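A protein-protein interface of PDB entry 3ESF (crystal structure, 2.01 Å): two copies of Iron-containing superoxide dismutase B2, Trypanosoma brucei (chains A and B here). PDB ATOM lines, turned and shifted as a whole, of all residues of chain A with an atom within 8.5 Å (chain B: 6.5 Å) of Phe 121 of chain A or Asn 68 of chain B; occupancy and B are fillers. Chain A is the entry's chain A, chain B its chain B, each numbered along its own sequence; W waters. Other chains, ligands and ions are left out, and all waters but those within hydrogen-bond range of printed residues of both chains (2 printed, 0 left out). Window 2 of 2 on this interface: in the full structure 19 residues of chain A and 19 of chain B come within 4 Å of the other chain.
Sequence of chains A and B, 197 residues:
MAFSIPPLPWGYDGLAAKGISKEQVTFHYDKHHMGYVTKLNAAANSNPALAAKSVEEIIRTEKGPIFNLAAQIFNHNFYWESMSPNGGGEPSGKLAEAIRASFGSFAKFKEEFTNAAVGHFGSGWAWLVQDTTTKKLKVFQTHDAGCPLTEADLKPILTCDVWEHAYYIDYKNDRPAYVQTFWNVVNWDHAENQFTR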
ATOM      1  N   ASN A 115      16.642 -32.487 -34.626  1.00  0.00           N
ATOM      2  CA  ASN A 115      17.090 -31.142 -35.022  1.00  0.00           C
ATOM      3  C   ASN A 115      17.241 -30.266 -33.774  1.00  0.00           C
ATOM      4  O   ASN A 115      18.205 -29.494 -33.642  1.00  0.00           O
ATOM      5  CB  ASN A 115      16.141 -30.522 -36.084  1.00  0.00           C
ATOM      6  CG  ASN A 115      16.409 -31.028 -37.524  1.00  0.00           C
ATOM      7  OD1 ASN A 115      15.626 -30.756 -38.448  1.00  0.00           O
ATOM      8  ND2 ASN A 115      17.484 -31.759 -37.716  1.00  0.00           N
ATOM      9  N   ALA A 116      16.313 -30.436 -32.824  1.00  0.00           N
ATOM     10  CA  ALA A 116      16.356 -29.708 -31.536  1.00  0.00           C
ATOM     11  C   ALA A 116      17.542 -30.129 -30.654  1.00  0.00           C
ATOM     12  O   ALA A 116      18.213 -29.283 -30.070  1.00  0.00           O
ATOM     13  CB  ALA A 116      15.026 -29.931 -30.753  1.00  0.00           C
ATOM     14  N   ALA A 117      17.752 -31.440 -30.528  1.00  0.00           N
ATOM     15  CA  ALA A 117      18.828 -31.985 -29.699  1.00  0.00           C
ATOM     16  C   ALA A 117      20.226 -31.651 -30.274  1.00  0.00           C
ATOM     17  O   ALA A 117      21.128 -31.299 -29.536  1.00  0.00           O
ATOM     18  CB  ALA A 117      18.668 -33.529 -29.514  1.00  0.00           C
ATOM     19  N   VAL A 118      20.376 -31.774 -31.586  1.00  0.00           N
ATOM     20  CA  VAL A 118      21.661 -31.550 -32.260  1.00  0.00           C
ATOM     21  C   VAL A 118      21.909 -30.063 -32.369  1.00  0.00           C
ATOM     22  O   VAL A 118      23.034 -29.593 -32.203  1.00  0.00           O
ATOM     23  CB  VAL A 118      21.698 -32.254 -33.631  1.00  0.00           C
ATOM     24  CG1 VAL A 118      22.877 -31.766 -34.499  1.00  0.00           C
ATOM     25  CG2 VAL A 118      21.773 -33.771 -33.436  1.00  0.00           C
ATOM     26  N   GLY A 119      20.846 -29.308 -32.583  1.00  0.00           N
ATOM     27  CA  GLY A 119      20.998 -27.869 -32.777  1.00  0.00           C
ATOM     28  C   GLY A 119      21.130 -27.045 -31.513  1.00  0.00           C
ATOM     29  O   GLY A 119      21.529 -25.891 -31.596  1.00  0.00           O
ATOM     30  N   HIS A 120      20.797 -27.590 -30.338  1.00  0.00           N
ATOM     31  CA  HIS A 120      20.800 -26.759 -29.128  1.00  0.00           C
ATOM     32  C   HIS A 120      22.193 -26.166 -28.880  1.00  0.00           C
ATOM     33  O   HIS A 120      23.157 -26.912 -28.840  1.00  0.00           O
ATOM     34  CB  HIS A 120      20.322 -27.527 -27.885  1.00  0.00           C
ATOM     35  CG  HIS A 120      20.041 -26.642 -26.706  1.00  0.00           C
ATOM     36  ND1 HIS A 120      18.811 -26.047 -26.503  1.00  0.00           N
ATOM     37  CD2 HIS A 120      20.841 -26.215 -25.693  1.00  0.00           C
ATOM     38  CE1 HIS A 120      18.868 -25.291 -25.416  1.00  0.00           C
ATOM     39  NE2 HIS A 120      20.083 -25.389 -24.900  1.00  0.00           N
ATOM     40  N   PHE A 121      22.292 -24.838 -28.726  1.00  0.00           N
ATOM     41  CA  PHE A 121      23.585 -24.189 -28.514  1.00  0.00           C
ATOM     42  C   PHE A 121      23.886 -24.046 -27.010  1.00  0.00           C
ATOM     43  O   PHE A 121      23.038 -23.584 -26.230  1.00  0.00           O
ATOM     44  CB  PHE A 121      23.643 -22.829 -29.219  1.00  0.00           C
ATOM     45  CG  PHE A 121      25.014 -22.200 -29.210  1.00  0.00           C
ATOM     46  CD1 PHE A 121      25.985 -22.596 -30.142  1.00  0.00           C
ATOM     47  CD2 PHE A 121      25.358 -21.227 -28.236  1.00  0.00           C
ATOM     48  CE1 PHE A 121      27.272 -22.018 -30.115  1.00  0.00           C
ATOM     49  CE2 PHE A 121      26.619 -20.669 -28.219  1.00  0.00           C
ATOM     50  CZ  PHE A 121      27.573 -21.068 -29.155  1.00  0.00           C
ATOM     51  N   GLY A 122      25.094 -24.447 -26.614  1.00  0.00           N
ATOM     52  CA  GLY A 122      25.469 -24.499 -25.195  1.00  0.00           C
ATOM     53  C   GLY A 122      24.764 -25.640 -24.478  1.00  0.00           C
ATOM     54  O   GLY A 122      24.391 -26.652 -25.098  1.00  0.00           O
ATOM     55  N   SER A 123      24.613 -25.482 -23.157  1.00  0.00           N
ATOM     56  CA  SER A 123      24.104 -26.541 -22.293  1.00  0.00           C
ATOM     57  C   SER A 123      22.579 -26.513 -22.281  1.00  0.00           C
ATOM     58  O   SER A 123      21.979 -25.422 -22.113  1.00  0.00           O
ATOM     59  CB  SER A 123      24.643 -26.389 -20.842  1.00  0.00           C
ATOM     60  OG  SER A 123      26.073 -26.311 -20.802  1.00  0.00           O
ATOM     61  N   GLY A 124      21.964 -27.676 -22.487  1.00  0.00           N
ATOM     62  CA  GLY A 124      20.488 -27.807 -22.391  1.00  0.00           C
ATOM     63  C   GLY A 124      19.898 -29.200 -22.571  1.00  0.00           C
ATOM     64  O   GLY A 124      20.574 -30.206 -22.404  1.00  0.00           O
ATOM     65  N   TRP A 125      18.608 -29.240 -22.926  1.00  0.00           N
ATOM     66  CA  TRP A 125      17.783 -30.441 -22.859  1.00  0.00           C
ATOM     67  C   TRP A 125      16.787 -30.400 -24.017  1.00  0.00           C
ATOM     68  O   TRP A 125      16.180 -29.352 -24.258  1.00  0.00           O
ATOM     69  CB  TRP A 125      16.967 -30.475 -21.555  1.00  0.00           C
ATOM     70  CG  TRP A 125      17.787 -30.486 -20.323  1.00  0.00           C
ATOM     71  CD1 TRP A 125      18.330 -29.397 -19.683  1.00  0.00           C
ATOM     72  CD2 TRP A 125      18.169 -31.631 -19.578  1.00  0.00           C
ATOM     73  NE1 TRP A 125      19.049 -29.805 -18.601  1.00  0.00           N
ATOM     74  CE2 TRP A 125      18.971 -31.173 -18.503  1.00  0.00           C
ATOM     75  CE3 TRP A 125      17.923 -33.007 -19.711  1.00  0.00           C
ATOM     76  CZ2 TRP A 125      19.520 -32.037 -17.561  1.00  0.00           C
ATOM     77  CZ3 TRP A 125      18.507 -33.879 -18.769  1.00  0.00           C
ATOM     78  CH2 TRP A 125      19.293 -33.377 -17.719  1.00  0.00           C
ATOM     79  N   GLN A 141      12.571 -27.268 -26.150  1.00  0.00           N
ATOM     80  CA  GLN A 141      13.927 -27.226 -25.594  1.00  0.00           C
ATOM     81  C   GLN A 141      13.957 -26.426 -24.281  1.00  0.00           C
ATOM     82  O   GLN A 141      13.222 -25.461 -24.102  1.00  0.00           O
ATOM     83  CB  GLN A 141      14.897 -26.580 -26.601  1.00  0.00           C
ATOM     84  CG  GLN A 141      15.029 -27.359 -27.879  1.00  0.00           C
ATOM     85  CD  GLN A 141      15.801 -26.611 -28.943  1.00  0.00           C
ATOM     86  OE1 GLN A 141      16.954 -26.209 -28.747  1.00  0.00           O
ATOM     87  NE2 GLN A 141      15.174 -26.436 -30.093  1.00  0.00           N
ATOM     88  N   THR A 142      14.836 -26.820 -23.370  1.00  0.00           N
ATOM     89  CA  THR A 142      15.225 -25.924 -22.288  1.00  0.00           C
ATOM     90  C   THR A 142      16.743 -25.743 -22.304  1.00  0.00           C
ATOM     91  O   THR A 142      17.486 -26.620 -22.761  1.00  0.00           O
ATOM     92  CB  THR A 142      14.757 -26.424 -20.919  1.00  0.00           C
ATOM     93  OG1 THR A 142      15.322 -27.714 -20.644  1.00  0.00           O
ATOM     94  CG2 THR A 142      13.226 -26.517 -20.870  1.00  0.00           C
ATOM     95  N   HIS A 143      17.189 -24.617 -21.779  1.00  0.00           N
ATOM     96  CA  HIS A 143      18.593 -24.245 -21.775  1.00  0.00           C
ATOM     97  C   HIS A 143      19.087 -24.328 -20.329  1.00  0.00           C
ATOM     98  O   HIS A 143      18.319 -24.018 -19.380  1.00  0.00           O
ATOM     99  CB  HIS A 143      18.736 -22.822 -22.305  1.00  0.00           C
ATOM    100  CG  HIS A 143      20.148 -22.418 -22.609  1.00  0.00           C
ATOM    101  ND1 HIS A 143      20.974 -23.154 -23.428  1.00  0.00           N
ATOM    102  CD2 HIS A 143      20.856 -21.319 -22.250  1.00  0.00           C
ATOM    103  CE1 HIS A 143      22.145 -22.538 -23.541  1.00  0.00           C
ATOM    104  NE2 HIS A 143      22.098 -21.425 -22.833  1.00  0.00           N
ATOM    105  N   ASP A 144      20.337 -24.742 -20.167  1.00  0.00           N
ATOM    106  CA  ASP A 144      20.947 -24.919 -18.819  1.00  0.00           C
ATOM    107  C   ASP A 144      20.114 -25.858 -17.929  1.00  0.00           C
ATOM    108  O   ASP A 144      20.015 -27.050 -18.228  1.00  0.00           O
ATOM    109  CB  ASP A 144      21.213 -23.558 -18.168  1.00  0.00           C
ATOM    110  CG  ASP A 144      22.111 -22.699 -19.019  1.00  0.00           C
ATOM    111  OD1 ASP A 144      23.106 -23.262 -19.541  1.00  0.00           O
ATOM    112  OD2 ASP A 144      21.821 -21.488 -19.170  1.00  0.00           O
ATOM    113  N   VAL A 162      21.603 -32.805 -23.381  1.00  0.00           N
ATOM    114  CA  VAL A 162      22.636 -32.430 -24.391  1.00  0.00           C
ATOM    115  C   VAL A 162      23.721 -31.485 -23.841  1.00  0.00           C
ATOM    116  O   VAL A 162      24.480 -30.877 -24.603  1.00  0.00           O
ATOM    117  CB  VAL A 162      22.035 -31.911 -25.720  1.00  0.00           C
ATOM    118  CG1 VAL A 162      21.140 -32.952 -26.338  1.00  0.00           C
ATOM    119  CG2 VAL A 162      21.289 -30.547 -25.530  1.00  0.00           C
ATOM    120  N   GLU A 164      27.335 -31.162 -22.606  1.00  0.00           N
ATOM    121  CA  GLU A 164      28.471 -31.868 -23.125  1.00  0.00           C
ATOM    122  C   GLU A 164      28.897 -33.053 -22.260  1.00  0.00           C
ATOM    123  O   GLU A 164      29.367 -34.042 -22.803  1.00  0.00           O
ATOM    124  CB  GLU A 164      29.643 -30.931 -23.418  1.00  0.00           C
ATOM    125  CG  GLU A 164      29.386 -30.143 -24.685  1.00  0.00           C
ATOM    126  CD  GLU A 164      30.365 -29.014 -24.958  1.00  0.00           C
ATOM    127  OE1 GLU A 164      30.933 -28.435 -24.030  1.00  0.00           O
ATOM    128  OE2 GLU A 164      30.575 -28.687 -26.134  1.00  0.00           O
ATOM    129  N   ARG A 175      28.033 -34.899 -31.005  1.00  0.00           N
ATOM    130  CA  ARG A 175      26.689 -34.948 -30.453  1.00  0.00           C
ATOM    131  C   ARG A 175      25.676 -35.575 -31.433  1.00  0.00           C
ATOM    132  O   ARG A 175      24.760 -36.249 -30.986  1.00  0.00           O
ATOM    133  CB  ARG A 175      26.223 -33.551 -30.010  1.00  0.00           C
ATOM    134  CG  ARG A 175      24.919 -33.628 -29.199  1.00  0.00           C
ATOM    135  CD  ARG A 175      24.120 -32.341 -29.121  1.00  0.00           C
ATOM    136  NE  ARG A 175      24.828 -31.233 -28.490  1.00  0.00           N
ATOM    137  CZ  ARG A 175      24.316 -30.011 -28.360  1.00  0.00           C
ATOM    138  NH1 ARG A 175      23.090 -29.721 -28.810  1.00  0.00           N
ATOM    139  NH2 ARG A 175      25.014 -29.075 -27.781  1.00  0.00           N
ATOM    140  N   TYR B  36      33.324 -24.074 -35.745  1.00  0.00           N
ATOM    141  CA  TYR B  36      32.671 -22.747 -35.865  1.00  0.00           C
ATOM    142  C   TYR B  36      33.031 -22.079 -37.171  1.00  0.00           C
ATOM    143  O   TYR B  36      32.171 -21.496 -37.806  1.00  0.00           O
ATOM    144  CB  TYR B  36      33.049 -21.809 -34.697  1.00  0.00           C
ATOM    145  CG  TYR B  36      32.617 -22.327 -33.332  1.00  0.00           C
ATOM    146  CD1 TYR B  36      31.264 -22.581 -33.061  1.00  0.00           C
ATOM    147  CD2 TYR B  36      33.545 -22.532 -32.323  1.00  0.00           C
ATOM    148  CE1 TYR B  36      30.860 -23.063 -31.815  1.00  0.00           C
ATOM    149  CE2 TYR B  36      33.160 -22.993 -31.056  1.00  0.00           C
ATOM    150  CZ  TYR B  36      31.821 -23.247 -30.820  1.00  0.00           C
ATOM    151  OH  TYR B  36      31.427 -23.708 -29.587  1.00  0.00           O
ATOM    152  N   ILE B  58      31.270  -8.677 -37.060  1.00  0.00           N
ATOM    153  CA  ILE B  58      30.127  -9.546 -36.895  1.00  0.00           C
ATOM    154  C   ILE B  58      29.661  -9.576 -35.442  1.00  0.00           C
ATOM    155  O   ILE B  58      28.452  -9.510 -35.179  1.00  0.00           O
ATOM    156  CB  ILE B  58      30.424 -10.978 -37.411  1.00  0.00           C
ATOM    157  CG1 ILE B  58      30.691 -10.943 -38.940  1.00  0.00           C
ATOM    158  CG2 ILE B  58      29.277 -11.943 -37.020  1.00  0.00           C
ATOM    159  CD1 ILE B  58      31.450 -12.200 -39.455  1.00  0.00           C
ATOM    160  N   LYS B  63      23.336 -10.788 -35.007  1.00  0.00           N
ATOM    161  CA  LYS B  63      22.552 -11.431 -33.932  1.00  0.00           C
ATOM    162  C   LYS B  63      22.267 -12.893 -34.283  1.00  0.00           C
ATOM    163  O   LYS B  63      22.364 -13.261 -35.457  1.00  0.00           O
ATOM    164  CB  LYS B  63      21.226 -10.661 -33.755  1.00  0.00           C
ATOM    165  CG  LYS B  63      21.415  -9.137 -33.534  1.00  0.00           C
ATOM    166  CD  LYS B  63      22.195  -8.871 -32.229  1.00  0.00           C
ATOM    167  CE  LYS B  63      22.552  -7.369 -32.117  1.00  0.00           C
ATOM    168  NZ  LYS B  63      23.560  -7.093 -31.009  1.00  0.00           N
ATOM    169  N   GLY B  64      21.915 -13.709 -33.288  1.00  0.00           N
ATOM    170  CA  GLY B  64      21.548 -15.120 -33.497  1.00  0.00           C
ATOM    171  C   GLY B  64      22.710 -16.057 -33.819  1.00  0.00           C
ATOM    172  O   GLY B  64      23.851 -15.782 -33.423  1.00  0.00           O
ATOM    173  N   PRO B  65      22.430 -17.176 -34.542  1.00  0.00           N
ATOM    174  CA  PRO B  65      23.475 -18.178 -34.779  1.00  0.00           C
ATOM    175  C   PRO B  65      24.752 -17.618 -35.412  1.00  0.00           C
ATOM    176  O   PRO B  65      25.827 -18.052 -35.061  1.00  0.00           O
ATOM    177  CB  PRO B  65      22.811 -19.167 -35.743  1.00  0.00           C
ATOM    178  CG  PRO B  65      21.339 -19.092 -35.381  1.00  0.00           C
ATOM    179  CD  PRO B  65      21.150 -17.586 -35.153  1.00  0.00           C
ATOM    180  N   ILE B  66      24.643 -16.661 -36.328  1.00  0.00           N
ATOM    181  CA  ILE B  66      25.845 -16.095 -36.978  1.00  0.00           C
ATOM    182  C   ILE B  66      26.722 -15.346 -35.955  1.00  0.00           C
ATOM    183  O   ILE B  66      27.952 -15.429 -35.986  1.00  0.00           O
ATOM    184  CB  ILE B  66      25.468 -15.158 -38.175  1.00  0.00           C
ATOM    185  CG1 ILE B  66      24.956 -15.949 -39.395  1.00  0.00           C
ATOM    186  CG2 ILE B  66      26.609 -14.211 -38.584  1.00  0.00           C
ATOM    187  CD1 ILE B  66      25.539 -17.362 -39.546  1.00  0.00           C
ATOM    188  N   PHE B  67      26.078 -14.569 -35.080  1.00  0.00           N
ATOM    189  CA  PHE B  67      26.779 -13.989 -33.947  1.00  0.00           C
ATOM    190  C   PHE B  67      27.518 -15.059 -33.130  1.00  0.00           C
ATOM    191  O   PHE B  67      28.704 -14.896 -32.809  1.00  0.00           O
ATOM    192  CB  PHE B  67      25.846 -13.197 -33.014  1.00  0.00           C
ATOM    193  CG  PHE B  67      26.494 -12.846 -31.703  1.00  0.00           C
ATOM    194  CD1 PHE B  67      27.257 -11.666 -31.583  1.00  0.00           C
ATOM    195  CD2 PHE B  67      26.430 -13.709 -30.613  1.00  0.00           C
ATOM    196  CE1 PHE B  67      27.885 -11.338 -30.391  1.00  0.00           C
ATOM    197  CE2 PHE B  67      27.086 -13.392 -29.404  1.00  0.00           C
ATOM    198  CZ  PHE B  67      27.811 -12.197 -29.302  1.00  0.00           C
ATOM    199  N   ASN B  68      26.809 -16.122 -32.740  1.00  0.00           N
ATOM    200  CA  ASN B  68      27.425 -17.186 -31.912  1.00  0.00           C
ATOM    201  C   ASN B  68      28.699 -17.738 -32.515  1.00  0.00           C
ATOM    202  O   ASN B  68      29.662 -17.967 -31.787  1.00  0.00           O
ATOM    203  CB  ASN B  68      26.446 -18.362 -31.649  1.00  0.00           C
ATOM    204  CG  ASN B  68      25.268 -17.977 -30.711  1.00  0.00           C
ATOM    205  OD1 ASN B  68      24.289 -18.701 -30.630  1.00  0.00           O
ATOM    206  ND2 ASN B  68      25.389 -16.876 -29.995  1.00  0.00           N
ATOM    207  N   LEU B  69      28.686 -17.966 -33.831  1.00  0.00           N
ATOM    208  CA  LEU B  69      29.825 -18.516 -34.594  1.00  0.00           C
ATOM    209  C   LEU B  69      31.021 -17.549 -34.531  1.00  0.00           C
ATOM    210  O   LEU B  69      32.103 -17.919 -34.072  1.00  0.00           O
ATOM    211  CB  LEU B  69      29.419 -18.769 -36.054  1.00  0.00           C
ATOM    212  CG  LEU B  69      28.367 -19.865 -36.294  1.00  0.00           C
ATOM    213  CD1 LEU B  69      27.993 -20.074 -37.823  1.00  0.00           C
ATOM    214  CD2 LEU B  69      28.834 -21.181 -35.629  1.00  0.00           C
ATOM    215  N   ALA B  70      30.809 -16.294 -34.963  1.00  0.00           N
ATOM    216  CA  ALA B  70      31.900 -15.297 -34.902  1.00  0.00           C
ATOM    217  C   ALA B  70      32.437 -15.092 -33.455  1.00  0.00           C
ATOM    218  O   ALA B  70      33.643 -15.022 -33.236  1.00  0.00           O
ATOM    219  CB  ALA B  70      31.463 -14.004 -35.501  1.00  0.00           C
ATOM    220  N   ALA B  71      31.530 -14.972 -32.489  1.00  0.00           N
ATOM    221  CA  ALA B  71      31.925 -14.749 -31.094  1.00  0.00           C
ATOM    222  C   ALA B  71      32.738 -15.898 -30.563  1.00  0.00           C
ATOM    223  O   ALA B  71      33.754 -15.668 -29.904  1.00  0.00           O
ATOM    224  CB  ALA B  71      30.705 -14.485 -30.204  1.00  0.00           C
ATOM    225  N   GLN B  72      32.324 -17.129 -30.877  1.00  0.00           N
ATOM    226  CA  GLN B  72      33.102 -18.329 -30.466  1.00  0.00           C
ATOM    227  C   GLN B  72      34.468 -18.381 -31.120  1.00  0.00           C
ATOM    228  O   GLN B  72      35.429 -18.820 -30.528  1.00  0.00           O
ATOM    229  CB  GLN B  72      32.335 -19.624 -30.755  1.00  0.00           C
ATOM    230  CG  GLN B  72      31.151 -19.911 -29.800  1.00  0.00           C
ATOM    231  CD  GLN B  72      31.601 -20.005 -28.322  1.00  0.00           C
ATOM    232  OE1 GLN B  72      31.845 -18.993 -27.670  1.00  0.00           O
ATOM    233  NE2 GLN B  72      31.720 -21.210 -27.816  1.00  0.00           N
ATOM    234  N   ILE B  73      34.544 -17.947 -32.368  1.00  0.00           N
ATOM    235  CA  ILE B  73      35.851 -17.821 -33.064  1.00  0.00           C
ATOM    236  C   ILE B  73      36.825 -16.875 -32.354  1.00  0.00           C
ATOM    237  O   ILE B  73      37.961 -17.253 -32.033  1.00  0.00           O
ATOM    238  CB  ILE B  73      35.644 -17.465 -34.546  1.00  0.00           C
ATOM    239  CG1 ILE B  73      35.035 -18.693 -35.260  1.00  0.00           C
ATOM    240  CG2 ILE B  73      36.968 -17.033 -35.205  1.00  0.00           C
ATOM    241  CD1 ILE B  73      34.473 -18.435 -36.633  1.00  0.00           C
ATOM    242  N   SER B 123      27.448 -23.459 -19.901  1.00  0.00           N
ATOM    243  CA  SER B 123      28.538 -23.115 -20.817  1.00  0.00           C
ATOM    244  C   SER B 123      28.867 -21.620 -20.732  1.00  0.00           C
ATOM    245  O   SER B 123      27.977 -20.794 -20.800  1.00  0.00           O
ATOM    246  CB  SER B 123      28.129 -23.421 -22.277  1.00  0.00           C
ATOM    247  OG  SER B 123      27.947 -24.809 -22.541  1.00  0.00           O
ATOM    248  N   HIS B 143      28.123 -15.936 -20.936  1.00  0.00           N
ATOM    249  CA  HIS B 143      27.454 -17.234 -20.977  1.00  0.00           C
ATOM    250  C   HIS B 143      27.357 -17.624 -22.444  1.00  0.00           C
ATOM    251  O   HIS B 143      27.195 -16.761 -23.295  1.00  0.00           O
ATOM    252  CB  HIS B 143      26.068 -17.084 -20.338  1.00  0.00           C
ATOM    253  CG  HIS B 143      25.349 -18.375 -20.092  1.00  0.00           C
ATOM    254  ND1 HIS B 143      25.913 -19.421 -19.393  1.00  0.00           N
ATOM    255  CD2 HIS B 143      24.083 -18.760 -20.394  1.00  0.00           C
ATOM    256  CE1 HIS B 143      25.037 -20.400 -19.291  1.00  0.00           C
ATOM    257  NE2 HIS B 143      23.922 -20.029 -19.895  1.00  0.00           N
ATOM    258  N   ASP B 144      27.512 -18.917 -22.727  1.00  0.00           N
ATOM    259  CA  ASP B 144      27.451 -19.463 -24.084  1.00  0.00           C
ATOM    260  C   ASP B 144      28.518 -18.837 -24.991  1.00  0.00           C
ATOM    261  O   ASP B 144      29.729 -19.002 -24.747  1.00  0.00           O
ATOM    262  CB  ASP B 144      26.005 -19.358 -24.663  1.00  0.00           C
ATOM    263  CG  ASP B 144      24.984 -20.147 -23.832  1.00  0.00           C
ATOM    264  OD1 ASP B 144      25.286 -21.293 -23.425  1.00  0.00           O
ATOM    265  OD2 ASP B 144      23.866 -19.625 -23.581  1.00  0.00           O
ATOM    266  N   ALA B 145      28.097 -18.087 -26.005  1.00  0.00           N
ATOM    267  CA  ALA B 145      29.031 -17.429 -26.912  1.00  0.00           C
ATOM    268  C   ALA B 145      29.218 -15.946 -26.576  1.00  0.00           C
ATOM    269  O   ALA B 145      29.783 -15.216 -27.372  1.00  0.00           O
ATOM    270  CB  ALA B 145      28.539 -17.579 -28.360  1.00  0.00           C
ATOM    271  N   GLY B 146      28.689 -15.485 -25.432  1.00  0.00           N
ATOM    272  CA  GLY B 146      28.729 -14.046 -25.093  1.00  0.00           C
ATOM    273  C   GLY B 146      30.169 -13.542 -25.167  1.00  0.00           C
ATOM    274  O   GLY B 146      31.108 -14.269 -24.873  1.00  0.00           O
ATOM    275  N   TRP B 163      33.222 -23.870 -20.916  1.00  0.00           N
ATOM    276  CA  TRP B 163      32.483 -24.914 -21.600  1.00  0.00           C
ATOM    277  C   TRP B 163      33.093 -26.269 -21.212  1.00  0.00           C
ATOM    278  O   TRP B 163      34.315 -26.402 -21.192  1.00  0.00           O
ATOM    279  CB  TRP B 163      32.572 -24.764 -23.124  1.00  0.00           C
ATOM    280  CG  TRP B 163      31.717 -23.697 -23.725  1.00  0.00           C
ATOM    281  CD1 TRP B 163      31.789 -22.355 -23.478  1.00  0.00           C
ATOM    282  CD2 TRP B 163      30.716 -23.856 -24.757  1.00  0.00           C
ATOM    283  NE1 TRP B 163      30.879 -21.674 -24.246  1.00  0.00           N
ATOM    284  CE2 TRP B 163      30.209 -22.566 -25.044  1.00  0.00           C
ATOM    285  CE3 TRP B 163      30.166 -24.968 -25.428  1.00  0.00           C
ATOM    286  CZ2 TRP B 163      29.171 -22.352 -25.968  1.00  0.00           C
ATOM    287  CZ3 TRP B 163      29.165 -24.750 -26.368  1.00  0.00           C
ATOM    288  CH2 TRP B 163      28.681 -23.454 -26.632  1.00  0.00           C
HETATM  289  O   HOH W   1      24.877 -23.205 -21.440  1.00  0.00           O
HETATM  290  O   HOH W   2      29.530 -26.936 -22.164  1.00  0.00           O
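Phe 121 of chain A touches just these residues of chain B: Asn 68, Gln 72, Asp 144, Ala 145 and Trp 163.
Asn 68 of chain B touches one residue of chain A.
Printed residues of chain A within 4 Å of Ala 145 of chain B: Phe 121 (3.6 Å).
Of the printed residues of chain A, Gln 72 of chain B touches Phe 121 (3.8 Å).
Of the printed residues of chain A, His 143 of chain B touches His 143 and Asp 144.
Of the printed residues of chain B, Gly 122 of chain A touches Ser 123, Asp 144 and Trp 163.
Gly 119 of chain A touches none of the printed residues of chain B.
Val 118 of chain A touches none of the printed residues of chain B.
Among the printed residues, merely in contact across the chains: Phe 121 of chain A with Asn 68 of chain B (3.6 Å), Phe 121 of chain A with Gln 72 of chain B (3.8 Å), Phe 121 of chain A with Asp 144 of chain B (3.8 Å), Phe 121 of chain A with Ala 145 of chain B (3.6 Å), Phe 121 of chain A with Trp 163 of chain B (3.6 Å), Gly 122 of chain A with Ser 123 of chain B (3.6 Å), Gly 122 of chain A with Asp 144 of chain B (3.7 Å), Gly 122 of chain A with Trp 163 of chain B (3.7 Å), His 143 of chain A with His 143 of chain B (3.7 Å) and Glu 164 of chain A with Trp 163 of chain B (3.8 Å).
The side-chain hydroxyl of Ser 123 of chain A sits at hydrogen-bond distance from the side-chain hydroxyl of Ser 123 of chain B, 3.0 Å away.
The side-chain carboxylate (OD2) of Asp 144 of chain A is in hydrogen-bond range of a ring nitrogen (NE2) of His 143 of chain B (2.7 Å).
A ring nitrogen (NE2) of His 143 of chain A sits at hydrogen-bond distance from the side-chain carboxylate of Asp 144 of chain B, at 2.6 Å.
Of the 19 printed residues of chain B, 7 touch a printed residue of chain A.
Printed residues of chain B that touch a printed residue of chain A: Asn 68, Gln 72, Ser 123, His 143, Asp 144, Ala 145 and Trp 163.
Hydrophobic or aromatic side chains of chain B that line the printed part of chain A: His 143, Ala 145 and Trp 163.
Of the 18 printed residues of chain A, 6 touch a printed residue of chain B.
Hydrophobic or aromatic side chains of chain A within 4 Å of the printed part of chain B: Phe 121 and His 143.
Along chain A the printed residues that touch a printed residue of chain B span positions 121 to 164.
The backbone carbonyl oxygen (O) of Ser 123 of chain A sits at hydrogen-bond distance from the backbone NH (N) of Asp 144 of chain A (2.6 Å).
O of Asp 144 of chain A sits at hydrogen-bond distance from NE1 of Trp 125 of chain A, at 2.9 Å.
O of Ser 123 of chain A sits at hydrogen-bond distance from NE2 of His 120 of chain A, at 3.4 Å.
NE2 of Gln 72 of chain B lies within hydrogen-bond range of OH of Tyr 36 of chain B (3.1 Å).
The backbone carbonyl oxygen (O) of Asp 144 of chain B sits at hydrogen-bond distance from the indole nitrogen (NE1) of Trp 163 of chain B, at 3.0 Å.
The backbone carbonyl oxygen (O) of Ser 123 of chain B sits at hydrogen-bond distance from the backbone NH (N) of Asp 144 of chain B (2.7 Å).
Water W1 lies within hydrogen-bond range of OD1 of Asp 144 of chain A, OD1 of Asp 144 of chain B, N of Ser 123 of chain A and N of Ser 123 of chain B.
Water W2 lies within hydrogen-bond range of OG of Ser 123 of chain B and OE1 of Glu 164 of chain A.
Ser 123 of chain A touches its own counterpart, Ser 123 of chain B.
His 143 of chain B touches its own counterpart, His 143 of chain A.
His 143 of chain A touches Asp 144 of chain B, and with the chains exchanged Asp 144 of chain A touches His 143 of chain B.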
